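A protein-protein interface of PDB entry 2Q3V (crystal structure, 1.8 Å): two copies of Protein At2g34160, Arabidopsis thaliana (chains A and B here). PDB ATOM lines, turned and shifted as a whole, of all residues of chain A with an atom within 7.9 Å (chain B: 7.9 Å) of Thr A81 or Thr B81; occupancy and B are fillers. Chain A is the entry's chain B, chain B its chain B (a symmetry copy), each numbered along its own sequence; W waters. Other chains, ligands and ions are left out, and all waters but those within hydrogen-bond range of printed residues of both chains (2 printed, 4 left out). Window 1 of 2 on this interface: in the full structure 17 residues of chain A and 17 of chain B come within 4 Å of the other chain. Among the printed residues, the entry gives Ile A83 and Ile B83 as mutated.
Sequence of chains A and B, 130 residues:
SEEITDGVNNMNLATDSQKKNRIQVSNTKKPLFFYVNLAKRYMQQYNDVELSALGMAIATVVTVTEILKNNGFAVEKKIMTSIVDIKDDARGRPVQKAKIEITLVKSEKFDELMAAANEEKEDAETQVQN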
ATOM      1  N   ALA A  53       7.886 -26.146 -25.490  1.00  0.00           N
ATOM      2  CA  ALA A  53       9.188 -26.754 -25.210  1.00  0.00           C
ATOM      3  C   ALA A  53       8.974 -28.198 -24.806  1.00  0.00           C
ATOM      4  O   ALA A  53       7.895 -28.547 -24.328  1.00  0.00           O
ATOM      5  CB  ALA A  53       9.886 -26.004 -24.039  1.00  0.00           C
ATOM      6  N   GLY A  55      10.609 -31.696 -22.670  1.00  0.00           N
ATOM      7  CA  GLY A  55      11.441 -32.144 -21.570  1.00  0.00           C
ATOM      8  C   GLY A  55      12.261 -31.111 -20.845  1.00  0.00           C
ATOM      9  O   GLY A  55      11.700 -30.200 -20.241  1.00  0.00           O
ATOM     10  N   ILE A  58      11.374 -27.341 -20.863  1.00  0.00           N
ATOM     11  CA  ILE A  58      10.179 -26.786 -20.245  1.00  0.00           C
ATOM     12  C   ILE A  58      10.616 -25.769 -19.166  1.00  0.00           C
ATOM     13  O   ILE A  58       9.957 -24.759 -18.934  1.00  0.00           O
ATOM     14  CB  ILE A  58       9.319 -27.941 -19.645  1.00  0.00           C
ATOM     15  CG1 ILE A  58       8.526 -28.610 -20.803  1.00  0.00           C
ATOM     16  CG2 ILE A  58       8.414 -27.413 -18.528  1.00  0.00           C
ATOM     17  CD1 ILE A  58       7.583 -29.802 -20.394  1.00  0.00           C
ATOM     18  N   VAL A  62       8.950 -22.100 -18.645  1.00  0.00           N
ATOM     19  CA  VAL A  62       8.402 -21.869 -17.305  1.00  0.00           C
ATOM     20  C   VAL A  62       8.993 -20.558 -16.759  1.00  0.00           C
ATOM     21  O   VAL A  62       8.259 -19.674 -16.288  1.00  0.00           O
ATOM     22  CB  VAL A  62       8.763 -23.066 -16.370  1.00  0.00           C
ATOM     23  CG1 VAL A  62       8.661 -22.656 -14.891  1.00  0.00           C
ATOM     24  CG2 VAL A  62       7.824 -24.227 -16.673  1.00  0.00           C
ATOM     25  N   GLU A  66       7.216 -16.845 -15.938  1.00  0.00           N
ATOM     26  CA  GLU A  66       7.290 -16.287 -14.593  1.00  0.00           C
ATOM     27  C   GLU A  66       7.868 -14.891 -14.675  1.00  0.00           C
ATOM     28  O   GLU A  66       7.399 -13.970 -14.015  1.00  0.00           O
ATOM     29  CB  GLU A  66       8.166 -17.169 -13.700  1.00  0.00           C
ATOM     30  CG  GLU A  66       7.471 -18.535 -13.425  1.00  0.00           C
ATOM     31  CD  GLU A  66       8.293 -19.476 -12.545  1.00  0.00           C
ATOM     32  OE1 GLU A  66       9.552 -19.436 -12.604  1.00  0.00           O
ATOM     33  OE2 GLU A  66       7.688 -20.306 -11.826  1.00  0.00           O
ATOM     34  N   GLU A  76      -1.291 -14.881 -18.785  1.00  0.00           N
ATOM     35  CA  GLU A  76      -1.388 -16.122 -19.536  1.00  0.00           C
ATOM     36  C   GLU A  76      -2.856 -16.406 -19.905  1.00  0.00           C
ATOM     37  O   GLU A  76      -3.760 -16.152 -19.115  1.00  0.00           O
ATOM     38  CB  GLU A  76      -0.844 -17.304 -18.703  1.00  0.00           C
ATOM     39  CG  GLU A  76      -1.755 -17.799 -17.569  1.00  0.00           C
ATOM     40  CD  GLU A  76      -1.861 -16.863 -16.353  1.00  0.00           C
ATOM     41  OE1 GLU A  76      -1.290 -15.736 -16.353  1.00  0.00           O
ATOM     42  OE2 GLU A  76      -2.529 -17.276 -15.372  1.00  0.00           O
ATOM     43  N   LYS A  78      -3.433 -19.580 -21.774  1.00  0.00           N
ATOM     44  CA  LYS A  78      -3.442 -21.044 -21.823  1.00  0.00           C
ATOM     45  C   LYS A  78      -2.088 -21.587 -21.369  1.00  0.00           C
ATOM     46  O   LYS A  78      -1.061 -21.099 -21.826  1.00  0.00           O
ATOM     47  CB  LYS A  78      -3.746 -21.489 -23.278  1.00  0.00           C
ATOM     48  CG  LYS A  78      -3.543 -22.971 -23.581  1.00  0.00           C
ATOM     49  CD  LYS A  78      -4.470 -23.451 -24.701  1.00  0.00           C
ATOM     50  CE  LYS A  78      -4.416 -22.574 -25.942  1.00  0.00           C
ATOM     51  NZ  LYS A  78      -3.062 -22.577 -26.559  1.00  0.00           N
ATOM     52  N   ILE A  79      -2.075 -22.575 -20.466  1.00  0.00           N
ATOM     53  CA  ILE A  79      -0.822 -23.192 -19.997  1.00  0.00           C
ATOM     54  C   ILE A  79      -1.107 -24.693 -19.925  1.00  0.00           C
ATOM     55  O   ILE A  79      -1.886 -25.114 -19.089  1.00  0.00           O
ATOM     56  CB  ILE A  79      -0.394 -22.661 -18.607  1.00  0.00           C
ATOM     57  CG1 ILE A  79      -0.158 -21.162 -18.714  1.00  0.00           C
ATOM     58  CG2 ILE A  79       0.923 -23.341 -18.136  1.00  0.00           C
ATOM     59  CD1 ILE A  79       0.378 -20.541 -17.467  1.00  0.00           C
ATOM     60  N   MET A  80      -0.474 -25.460 -20.810  1.00  0.00           N
ATOM     61  CA  MET A  80      -0.720 -26.899 -20.935  1.00  0.00           C
ATOM     62  C   MET A  80       0.523 -27.752 -21.133  1.00  0.00           C
ATOM     63  O   MET A  80       1.393 -27.429 -21.962  1.00  0.00           O
ATOM     64  CB  MET A  80      -1.705 -27.145 -22.098  1.00  0.00           C
ATOM     65  CG  MET A  80      -1.731 -28.590 -22.583  1.00  0.00           C
ATOM     66  SD  MET A  80      -3.347 -29.546 -22.131  1.00  0.00           S
ATOM     67  CE  MET A  80      -3.126 -29.621 -20.222  1.00  0.00           C
ATOM     68  N   THR A  81       0.623 -28.835 -20.359  1.00  0.00           N
ATOM     69  CA  THR A  81       1.767 -29.743 -20.503  1.00  0.00           C
ATOM     70  C   THR A  81       1.184 -31.111 -20.805  1.00  0.00           C
ATOM     71  O   THR A  81       0.269 -31.548 -20.131  1.00  0.00           O
ATOM     72  CB  THR A  81       2.618 -29.839 -19.224  1.00  0.00           C
ATOM     73  OG1 THR A  81       3.043 -28.521 -18.824  1.00  0.00           O
ATOM     74  CG2 THR A  81       3.863 -30.730 -19.495  1.00  0.00           C
ATOM     75  N   SER A  82       1.693 -31.752 -21.845  1.00  0.00           N
ATOM     76  CA  SER A  82       1.187 -33.046 -22.264  1.00  0.00           C
ATOM     77  C   SER A  82       2.338 -34.015 -22.453  1.00  0.00           C
ATOM     78  O   SER A  82       3.495 -33.627 -22.364  1.00  0.00           O
ATOM     79  CB  SER A  82       0.460 -32.893 -23.587  1.00  0.00           C
ATOM     80  OG  SER A  82       1.326 -32.273 -24.516  1.00  0.00           O
ATOM     81  N   ILE A  83       1.994 -35.286 -22.663  1.00  0.00           N
ATOM     82  CA  ILE A  83       2.995 -36.301 -22.942  1.00  0.00           C
ATOM     83  C   ILE A  83       2.657 -36.852 -24.325  1.00  0.00           C
ATOM     84  O   ILE A  83       1.667 -37.592 -24.484  1.00  0.00           O
ATOM     85  CB  ILE A  83       2.946 -37.487 -21.919  1.00  0.00           C
ATOM     86  CG1 ILE A  83       3.022 -36.976 -20.481  1.00  0.00           C
ATOM     87  CG2 ILE A  83       4.091 -38.462 -22.185  1.00  0.00           C
ATOM     88  CD1 ILE A  83       4.162 -35.982 -20.186  1.00  0.00           C
ATOM     89  N   VAL A  84       3.451 -36.485 -25.325  1.00  0.00           N
ATOM     90  CA  VAL A  84       3.233 -36.964 -26.685  1.00  0.00           C
ATOM     91  C   VAL A  84       4.348 -37.919 -27.085  1.00  0.00           C
ATOM     92  O   VAL A  84       5.318 -38.115 -26.349  1.00  0.00           O
ATOM     93  CB  VAL A  84       3.227 -35.816 -27.717  1.00  0.00           C
ATOM     94  CG1 VAL A  84       2.215 -34.732 -27.288  1.00  0.00           C
ATOM     95  CG2 VAL A  84       4.596 -35.247 -27.861  1.00  0.00           C
ATOM     96  N   LYS A  97       7.809 -37.772 -24.466  1.00  0.00           N
ATOM     97  CA  LYS A  97       8.406 -36.608 -23.809  1.00  0.00           C
ATOM     98  C   LYS A  97       7.345 -35.670 -23.292  1.00  0.00           C
ATOM     99  O   LYS A  97       6.226 -35.641 -23.801  1.00  0.00           O
ATOM    100  CB  LYS A  97       9.270 -35.796 -24.793  1.00  0.00           C
ATOM    101  CG  LYS A  97      10.572 -36.483 -25.242  1.00  0.00           C
ATOM    102  CD  LYS A  97      11.541 -36.645 -24.051  1.00  0.00           C
ATOM    103  CE  LYS A  97      12.149 -35.296 -23.610  1.00  0.00           C
ATOM    104  NZ  LYS A  97      13.126 -35.485 -22.480  1.00  0.00           N
ATOM    105  N   ALA A  98       7.697 -34.883 -22.284  1.00  0.00           N
ATOM    106  CA  ALA A  98       6.738 -33.901 -21.825  1.00  0.00           C
ATOM    107  C   ALA A  98       6.871 -32.703 -22.799  1.00  0.00           C
ATOM    108  O   ALA A  98       7.980 -32.354 -23.242  1.00  0.00           O
ATOM    109  CB  ALA A  98       7.060 -33.453 -20.410  1.00  0.00           C
ATOM    110  N   LYS A  99       5.729 -32.104 -23.135  1.00  0.00           N
ATOM    111  CA  LYS A  99       5.674 -30.932 -24.009  1.00  0.00           C
ATOM    112  C   LYS A  99       4.789 -29.901 -23.313  1.00  0.00           C
ATOM    113  O   LYS A  99       3.742 -30.245 -22.774  1.00  0.00           O
ATOM    114  CB  LYS A  99       5.049 -31.294 -25.359  1.00  0.00           C
ATOM    115  CG  LYS A  99       4.803 -30.074 -26.260  1.00  0.00           C
ATOM    116  CD  LYS A  99       3.994 -30.449 -27.513  1.00  0.00           C
ATOM    117  CE  LYS A  99       3.636 -29.155 -28.282  1.00  0.00           C
ATOM    118  NZ  LYS A  99       2.896 -29.475 -29.523  1.00  0.00           N
ATOM    119  N   ILE A 100       5.219 -28.631 -23.301  1.00  0.00           N
ATOM    120  CA  ILE A 100       4.392 -27.599 -22.699  1.00  0.00           C
ATOM    121  C   ILE A 100       4.065 -26.586 -23.817  1.00  0.00           C
ATOM    122  O   ILE A 100       4.827 -26.442 -24.804  1.00  0.00           O
ATOM    123  CB  ILE A 100       5.135 -26.889 -21.506  1.00  0.00           C
ATOM    124  CG1 ILE A 100       4.149 -26.035 -20.679  1.00  0.00           C
ATOM    125  CG2 ILE A 100       6.234 -25.988 -22.022  1.00  0.00           C
ATOM    126  CD1 ILE A 100       4.790 -25.499 -19.402  1.00  0.00           C
ATOM    127  N   GLU A 101       2.929 -25.923 -23.683  1.00  0.00           N
ATOM    128  CA  GLU A 101       2.520 -24.908 -24.657  1.00  0.00           C
ATOM    129  C   GLU A 101       1.916 -23.784 -23.820  1.00  0.00           C
ATOM    130  O   GLU A 101       0.960 -24.001 -23.041  1.00  0.00           O
ATOM    131  CB  GLU A 101       1.475 -25.462 -25.648  1.00  0.00           C
ATOM    132  CG  GLU A 101       2.027 -26.460 -26.678  1.00  0.00           C
ATOM    133  CD  GLU A 101       1.006 -26.802 -27.779  1.00  0.00           C
ATOM    134  OE1 GLU A 101      -0.213 -26.798 -27.486  1.00  0.00           O
ATOM    135  OE2 GLU A 101       1.419 -27.086 -28.931  1.00  0.00           O
ATOM    136  N   ILE A 102       2.492 -22.585 -23.957  1.00  0.00           N
ATOM    137  CA  ILE A 102       2.014 -21.445 -23.206  1.00  0.00           C
ATOM    138  C   ILE A 102       1.737 -20.233 -24.058  1.00  0.00           C
ATOM    139  O   ILE A 102       2.648 -19.663 -24.659  1.00  0.00           O
ATOM    140  CB  ILE A 102       3.000 -21.056 -22.121  1.00  0.00           C
ATOM    141  CG1 ILE A 102       3.088 -22.240 -21.150  1.00  0.00           C
ATOM    142  CG2 ILE A 102       2.552 -19.721 -21.441  1.00  0.00           C
ATOM    143  CD1 ILE A 102       4.024 -22.040 -19.950  1.00  0.00           C
ATOM    144  N   ALA B  53       4.839 -29.693  -8.473  1.00  0.00           N
ATOM    145  CA  ALA B  53       6.107 -28.990  -8.273  1.00  0.00           C
ATOM    146  C   ALA B  53       5.951 -27.559  -8.746  1.00  0.00           C
ATOM    147  O   ALA B  53       5.095 -27.283  -9.585  1.00  0.00           O
ATOM    148  CB  ALA B  53       7.232 -29.672  -9.103  1.00  0.00           C
ATOM    149  N   GLY B  55       7.991 -23.925 -10.195  1.00  0.00           N
ATOM    150  CA  GLY B  55       9.129 -23.404 -10.928  1.00  0.00           C
ATOM    151  C   GLY B  55      10.227 -24.366 -11.295  1.00  0.00           C
ATOM    152  O   GLY B  55       9.988 -25.306 -12.048  1.00  0.00           O
ATOM    153  N   ILE B  58       9.666 -28.190 -11.547  1.00  0.00           N
ATOM    154  CA  ILE B  58       8.817 -28.820 -12.547  1.00  0.00           C
ATOM    155  C   ILE B  58       9.685 -29.789 -13.382  1.00  0.00           C
ATOM    156  O   ILE B  58       9.228 -30.840 -13.823  1.00  0.00           O
ATOM    157  CB  ILE B  58       8.151 -27.722 -13.432  1.00  0.00           C
ATOM    158  CG1 ILE B  58       6.948 -27.127 -12.647  1.00  0.00           C
ATOM    159  CG2 ILE B  58       7.749 -28.298 -14.793  1.00  0.00           C
ATOM    160  CD1 ILE B  58       6.133 -26.000 -13.384  1.00  0.00           C
ATOM    161  N   VAL B  62       8.586 -33.561 -14.419  1.00  0.00           N
ATOM    162  CA  VAL B  62       8.575 -33.813 -15.864  1.00  0.00           C
ATOM    163  C   VAL B  62       9.416 -35.070 -16.143  1.00  0.00           C
ATOM    164  O   VAL B  62       8.967 -35.998 -16.834  1.00  0.00           O
ATOM    165  CB  VAL B  62       9.163 -32.580 -16.622  1.00  0.00           C
ATOM    166  CG1 VAL B  62       9.630 -32.977 -18.032  1.00  0.00           C
ATOM    167  CG2 VAL B  62       8.098 -31.493 -16.693  1.00  0.00           C
ATOM    168  N   GLU B  66       8.325 -38.889 -17.499  1.00  0.00           N
ATOM    169  CA  GLU B  66       8.919 -39.423 -18.719  1.00  0.00           C
ATOM    170  C   GLU B  66       9.527 -40.775 -18.416  1.00  0.00           C
ATOM    171  O   GLU B  66       9.395 -41.718 -19.188  1.00  0.00           O
ATOM    172  CB  GLU B  66       9.992 -38.468 -19.248  1.00  0.00           C
ATOM    173  CG  GLU B  66       9.347 -37.153 -19.774  1.00  0.00           C
ATOM    174  CD  GLU B  66      10.362 -36.143 -20.310  1.00  0.00           C
ATOM    175  OE1 GLU B  66      11.514 -36.093 -19.802  1.00  0.00           O
ATOM    176  OE2 GLU B  66       9.998 -35.349 -21.210  1.00  0.00           O
ATOM    177  N   GLU B  76      -0.472 -41.495 -17.884  1.00  0.00           N
ATOM    178  CA  GLU B  76      -0.921 -40.275 -17.235  1.00  0.00           C
ATOM    179  C   GLU B  76      -2.441 -40.101 -17.424  1.00  0.00           C
ATOM    180  O   GLU B  76      -2.979 -40.409 -18.483  1.00  0.00           O
ATOM    181  CB  GLU B  76      -0.200 -39.046 -17.832  1.00  0.00           C
ATOM    182  CG  GLU B  76      -0.674 -38.602 -19.224  1.00  0.00           C
ATOM    183  CD  GLU B  76      -0.267 -39.527 -20.384  1.00  0.00           C
ATOM    184  OE1 GLU B  76       0.345 -40.610 -20.163  1.00  0.00           O
ATOM    185  OE2 GLU B  76      -0.564 -39.150 -21.545  1.00  0.00           O
ATOM    186  N   LYS B  78      -3.878 -37.003 -15.931  1.00  0.00           N
ATOM    187  CA  LYS B  78      -4.009 -35.544 -15.908  1.00  0.00           C
ATOM    188  C   LYS B  78      -2.625 -34.899 -15.851  1.00  0.00           C
ATOM    189  O   LYS B  78      -1.799 -35.318 -15.048  1.00  0.00           O
ATOM    190  CB  LYS B  78      -4.848 -35.141 -14.667  1.00  0.00           C
ATOM    191  CG  LYS B  78      -4.874 -33.652 -14.330  1.00  0.00           C
ATOM    192  CD  LYS B  78      -6.175 -33.255 -13.626  1.00  0.00           C
ATOM    193  CE  LYS B  78      -6.509 -34.143 -12.438  1.00  0.00           C
ATOM    194  NZ  LYS B  78      -5.473 -34.050 -11.374  1.00  0.00           N
ATOM    195  N   ILE B  79      -2.358 -33.900 -16.702  1.00  0.00           N
ATOM    196  CA  ILE B  79      -1.068 -33.189 -16.696  1.00  0.00           C
ATOM    197  C   ILE B  79      -1.414 -31.712 -16.886  1.00  0.00           C
ATOM    198  O   ILE B  79      -1.867 -31.336 -17.952  1.00  0.00           O
ATOM    199  CB  ILE B  79      -0.131 -33.670 -17.831  1.00  0.00           C
ATOM    200  CG1 ILE B  79       0.158 -35.149 -17.626  1.00  0.00           C
ATOM    201  CG2 ILE B  79       1.215 -32.891 -17.804  1.00  0.00           C
ATOM    202  CD1 ILE B  79       1.150 -35.714 -18.587  1.00  0.00           C
ATOM    203  N   MET B  80      -1.200 -30.913 -15.842  1.00  0.00           N
ATOM    204  CA  MET B  80      -1.577 -29.498 -15.834  1.00  0.00           C
ATOM    205  C   MET B  80      -0.553 -28.560 -15.212  1.00  0.00           C
ATOM    206  O   MET B  80      -0.020 -28.831 -14.121  1.00  0.00           O
ATOM    207  CB  MET B  80      -2.929 -29.339 -15.108  1.00  0.00           C
ATOM    208  CG  MET B  80      -3.232 -27.905 -14.684  1.00  0.00           C
ATOM    209  SD  MET B  80      -4.640 -27.061 -15.700  1.00  0.00           S
ATOM    210  CE  MET B  80      -3.752 -26.945 -17.402  1.00  0.00           C
ATOM    211  N   THR B  81      -0.258 -27.462 -15.912  1.00  0.00           N
ATOM    212  CA  THR B  81       0.689 -26.477 -15.378  1.00  0.00           C
ATOM    213  C   THR B  81      -0.060 -25.158 -15.324  1.00  0.00           C
ATOM    214  O   THR B  81      -0.700 -24.779 -16.289  1.00  0.00           O
ATOM    215  CB  THR B  81       1.934 -26.303 -16.265  1.00  0.00           C
ATOM    216  OG1 THR B  81       2.568 -27.582 -16.468  1.00  0.00           O
ATOM    217  CG2 THR B  81       2.931 -25.329 -15.576  1.00  0.00           C
ATOM    218  N   SER B  82      -0.008 -24.496 -14.180  1.00  0.00           N
ATOM    219  CA  SER B  82      -0.722 -23.248 -13.989  1.00  0.00           C
ATOM    220  C   SER B  82       0.211 -22.202 -13.411  1.00  0.00           C
ATOM    221  O   SER B  82       1.347 -22.504 -13.071  1.00  0.00           O
ATOM    222  CB  SER B  82      -1.864 -23.470 -13.015  1.00  0.00           C
ATOM    223  OG  SER B  82      -1.349 -24.039 -11.828  1.00  0.00           O
ATOM    224  N   ILE B  83      -0.275 -20.962 -13.356  1.00  0.00           N
ATOM    225  CA  ILE B  83       0.482 -19.881 -12.748  1.00  0.00           C
ATOM    226  C   ILE B  83      -0.370 -19.375 -11.587  1.00  0.00           C
ATOM    227  O   ILE B  83      -1.402 -18.709 -11.806  1.00  0.00           O
ATOM    228  CB  ILE B  83       0.720 -18.688 -13.736  1.00  0.00           C
ATOM    229  CG1 ILE B  83       1.346 -19.173 -15.043  1.00  0.00           C
ATOM    230  CG2 ILE B  83       1.620 -17.638 -13.088  1.00  0.00           C
ATOM    231  CD1 ILE B  83       2.583 -20.079 -14.894  1.00  0.00           C
ATOM    232  N   VAL B  84       0.034 -19.696 -10.364  1.00  0.00           N
ATOM    233  CA  VAL B  84      -0.693 -19.253  -9.181  1.00  0.00           C
ATOM    234  C   VAL B  84       0.131 -18.226  -8.418  1.00  0.00           C
ATOM    235  O   VAL B  84       1.285 -17.951  -8.757  1.00  0.00           O
ATOM    236  CB  VAL B  84      -0.989 -20.412  -8.205  1.00  0.00           C
ATOM    237  CG1 VAL B  84      -1.697 -21.560  -8.955  1.00  0.00           C
ATOM    238  CG2 VAL B  84       0.274 -20.883  -7.569  1.00  0.00           C
ATOM    239  N   LYS B  97       4.305 -18.089  -9.611  1.00  0.00           N
ATOM    240  CA  LYS B  97       5.180 -19.199  -9.994  1.00  0.00           C
ATOM    241  C   LYS B  97       4.447 -20.204 -10.846  1.00  0.00           C
ATOM    242  O   LYS B  97       3.224 -20.320 -10.774  1.00  0.00           O
ATOM    243  CB  LYS B  97       5.687 -19.961  -8.753  1.00  0.00           C
ATOM    244  CG  LYS B  97       6.687 -19.188  -7.875  1.00  0.00           C
ATOM    245  CD  LYS B  97       8.006 -18.941  -8.638  1.00  0.00           C
ATOM    246  CE  LYS B  97       8.826 -20.237  -8.812  1.00  0.00           C
ATOM    247  NZ  LYS B  97      10.130 -19.963  -9.517  1.00  0.00           N
ATOM    248  N   ALA B  98       5.194 -20.950 -11.649  1.00  0.00           N
ATOM    249  CA  ALA B  98       4.538 -21.992 -12.409  1.00  0.00           C
ATOM    250  C   ALA B  98       4.396 -23.191 -11.436  1.00  0.00           C
ATOM    251  O   ALA B  98       5.293 -23.464 -10.619  1.00  0.00           O
ATOM    252  CB  ALA B  98       5.379 -22.397 -13.607  1.00  0.00           C
ATOM    253  N   LYS B  99       3.256 -23.874 -11.527  1.00  0.00           N
ATOM    254  CA  LYS B  99       2.973 -25.059 -10.716  1.00  0.00           C
ATOM    255  C   LYS B  99       2.475 -26.141 -11.670  1.00  0.00           C
ATOM    256  O   LYS B  99       1.671 -25.866 -12.554  1.00  0.00           O
ATOM    257  CB  LYS B  99       1.880 -24.761  -9.686  1.00  0.00           C
ATOM    258  CG  LYS B  99       1.413 -26.007  -8.919  1.00  0.00           C
ATOM    259  CD  LYS B  99       0.183 -25.707  -8.047  1.00  0.00           C
ATOM    260  CE  LYS B  99      -0.335 -27.033  -7.441  1.00  0.00           C
ATOM    261  NZ  LYS B  99      -1.493 -26.784  -6.555  1.00  0.00           N
ATOM    262  N   ILE B 100       2.970 -27.376 -11.509  1.00  0.00           N
ATOM    263  CA  ILE B 100       2.492 -28.457 -12.355  1.00  0.00           C
ATOM    264  C   ILE B 100       1.857 -29.505 -11.417  1.00  0.00           C
ATOM    265  O   ILE B 100       2.220 -29.608 -10.220  1.00  0.00           O
ATOM    266  CB  ILE B 100       3.664 -29.096 -13.190  1.00  0.00           C
ATOM    267  CG1 ILE B 100       3.106 -30.007 -14.305  1.00  0.00           C
ATOM    268  CG2 ILE B 100       4.564 -29.923 -12.301  1.00  0.00           C
ATOM    269  CD1 ILE B 100       4.201 -30.478 -15.259  1.00  0.00           C
ATOM    270  N   GLU B 101       0.897 -30.247 -11.943  1.00  0.00           N
ATOM    271  CA  GLU B 101       0.238 -31.301 -11.167  1.00  0.00           C
ATOM    272  C   GLU B 101       0.058 -32.454 -12.151  1.00  0.00           C
ATOM    273  O   GLU B 101      -0.565 -32.296 -13.225  1.00  0.00           O
ATOM    274  CB  GLU B 101      -1.131 -30.837 -10.627  1.00  0.00           C
ATOM    275  CG  GLU B 101      -1.060 -29.815  -9.481  1.00  0.00           C
ATOM    276  CD  GLU B 101      -2.431 -29.562  -8.827  1.00  0.00           C
ATOM    277  OE1 GLU B 101      -3.459 -29.649  -9.539  1.00  0.00           O
ATOM    278  OE2 GLU B 101      -2.482 -29.265  -7.607  1.00  0.00           O
ATOM    279  N   ILE B 102       0.630 -33.610 -11.799  1.00  0.00           N
ATOM    280  CA  ILE B 102       0.538 -34.772 -12.657  1.00  0.00           C
ATOM    281  C   ILE B 102       0.061 -36.011 -11.946  1.00  0.00           C
ATOM    282  O   ILE B 102       0.732 -36.523 -11.050  1.00  0.00           O
ATOM    283  CB  ILE B 102       1.874 -35.074 -13.308  1.00  0.00           C
ATOM    284  CG1 ILE B 102       2.221 -33.875 -14.199  1.00  0.00           C
ATOM    285  CG2 ILE B 102       1.798 -36.429 -14.087  1.00  0.00           C
ATOM    286  CD1 ILE B 102       3.538 -33.990 -14.977  1.00  0.00           C
HETATM  287  O   HOH W   1      -0.709 -36.459 -22.124  1.00  0.00           O
HETATM  288  O   HOH W   2      -2.679 -19.978 -14.848  1.00  0.00           O
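Water W2 bridges the side-chain carboxylate of Glu A76 (2.8 Å) and the backbone NH of Ile B83 (3.0 Å). Water W1 lies within hydrogen-bond range of the side-chain carboxylate (OE2) of Glu B76 (2.8 Å) and the backbone NH (N) of Ile A83 (3.0 Å).
The side-chain carboxylate (OE1) of Glu A66 is in salt-bridge range of the side-chain amino group (NZ) of Lys B97. The side-chain carboxylate (OE2) of Glu A66 sits at hydrogen-bond distance from the backbone NH (N) of Ala B98, at 2.6 Å. The side-chain hydroxyl (OG1) of Thr A81 is in hydrogen-bond range of the side-chain hydroxyl (OG1) of Thr B81 (2.6 Å). The side-chain amino group (NZ) of Lys A97 lies within salt-bridge range of the side-chain carboxylate (OE1) of Glu B66, 3.2 Å away. The backbone NH (N) of Ala A98 lies within hydrogen-bond range of the side-chain carboxylate (OE2) of Glu B66, at 2.6 Å. The backbone carbonyl oxygen of Ile A79 sits close to the backbone carbonyl oxygen of Thr B81 (3.1 Å). O of Thr A81 lies close to O of Ile B79.
Ala A53 touches none of the printed residues of chain B. Printed residues of chain B within 4 Å of Ile A58: Ile B58 (3.9 Å). Of the printed residues of chain B, Glu A76 touches Ile B83 (3.9 Å). Thr A81 touches just these residues of chain B: Ile B79 (2.8 Å) and Thr B81 (2.6 Å). Of the printed residues of chain B, Ile A83 touches Glu B76 (3.9 Å) and Ile B79 (2.9 Å). Lys A99 touches none of the printed residues of chain B. Of the printed residues of chain A, Glu B76 touches Ile A83. Of chain A, only Ile A79 (2.8 Å) and Thr A81 (2.6 Å) come within 4 Å of Thr B81. The nearest residue of chain A that does not touch Thr B81 is Ile A100 (4.2 Å). The nearest printed residue of chain A that does not touch Glu B76 is Ser A82 (6.0 Å).
Among the printed residues, pairs that only touch across the chains: Ile A79 with Ile B83 (2.9 Å), Ile A83 with Ile B79 (2.9 Å), Met A80 with Ile B79 (3.1 Å), Ile A79 with Met B80 (3.1 Å), Glu A66 with Gly B55 (3.5 Å), Gly A55 with Glu B66 (3.5 Å), Ala A98 with Val B62 (3.5 Å), Val A62 with Ala B98 (3.5 Å), Ile A58 with Ile B58 (3.9 Å), Ile A83 with Glu B76 (3.9 Å), Glu A76 with Ile B83 (3.9 Å) and Met A80 with Met B80 (3.9 Å).
O of Ala A98 sits at hydrogen-bond distance from N of Gly A55 (2.8 Å). The backbone carbonyl oxygen (O) of Met A80 lies within hydrogen-bond range of the backbone NH (N) of Glu A101. The backbone NH (N) of Lys A97 sits at hydrogen-bond distance from the backbone carbonyl oxygen (O) of Val A84. N of Gly B55 sits at hydrogen-bond distance from O of Ala B98, 2.8 Å away. O of Met B80 is in hydrogen-bond range of N of Glu B101. The backbone carbonyl oxygen (O) of Val B84 is in hydrogen-bond range of the backbone NH (N) of Lys B97, at 3.1 Å.
Glu A66 touches Lys B97, and with the chains exchanged Lys A97 touches Glu B66. Glu A66 touches Ala B98, and with the chains exchanged Ala A98 touches Glu B66. Glu A76 touches Ile B83, and with the chains exchanged Ile A83 touches Glu B76. Met B80 touches its own counterpart, Met A80. Positions printed for both chains: 53, 55, 58, 62, 66, 76, 78, 79, 80, 81, 82, 83, 84, 97, 98, 99, 100, 101 and 102. Of the 19 pairs that touch across the chains among the printed residues, 19 have their exchanged pair printed and touching as well.
Hydrophobic or aromatic side chains of chain A that line the printed part of chain B: Ile A58, Val A62, Ile A79, Met A80, Ile A83 and Ala A98. Of the 19 printed residues of chain B, 11 touch a printed residue of chain A. Hydrophobic or aromatic side chains of chain B within 4 Å of the printed part of chain A: Ile B58, Val B62, Ile B79, Met B80, Ile B83 and Ala B98. Among the printed residues, 19 pairs touch across the chains. Among the printed residues, Asp or Glu carboxylates within 4 Å of a Lys or Arg side-chain nitrogen of the other chain: Glu A66 with Lys B97 (3.2 Å) and Lys A97 with Glu B66 (3.2 Å).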
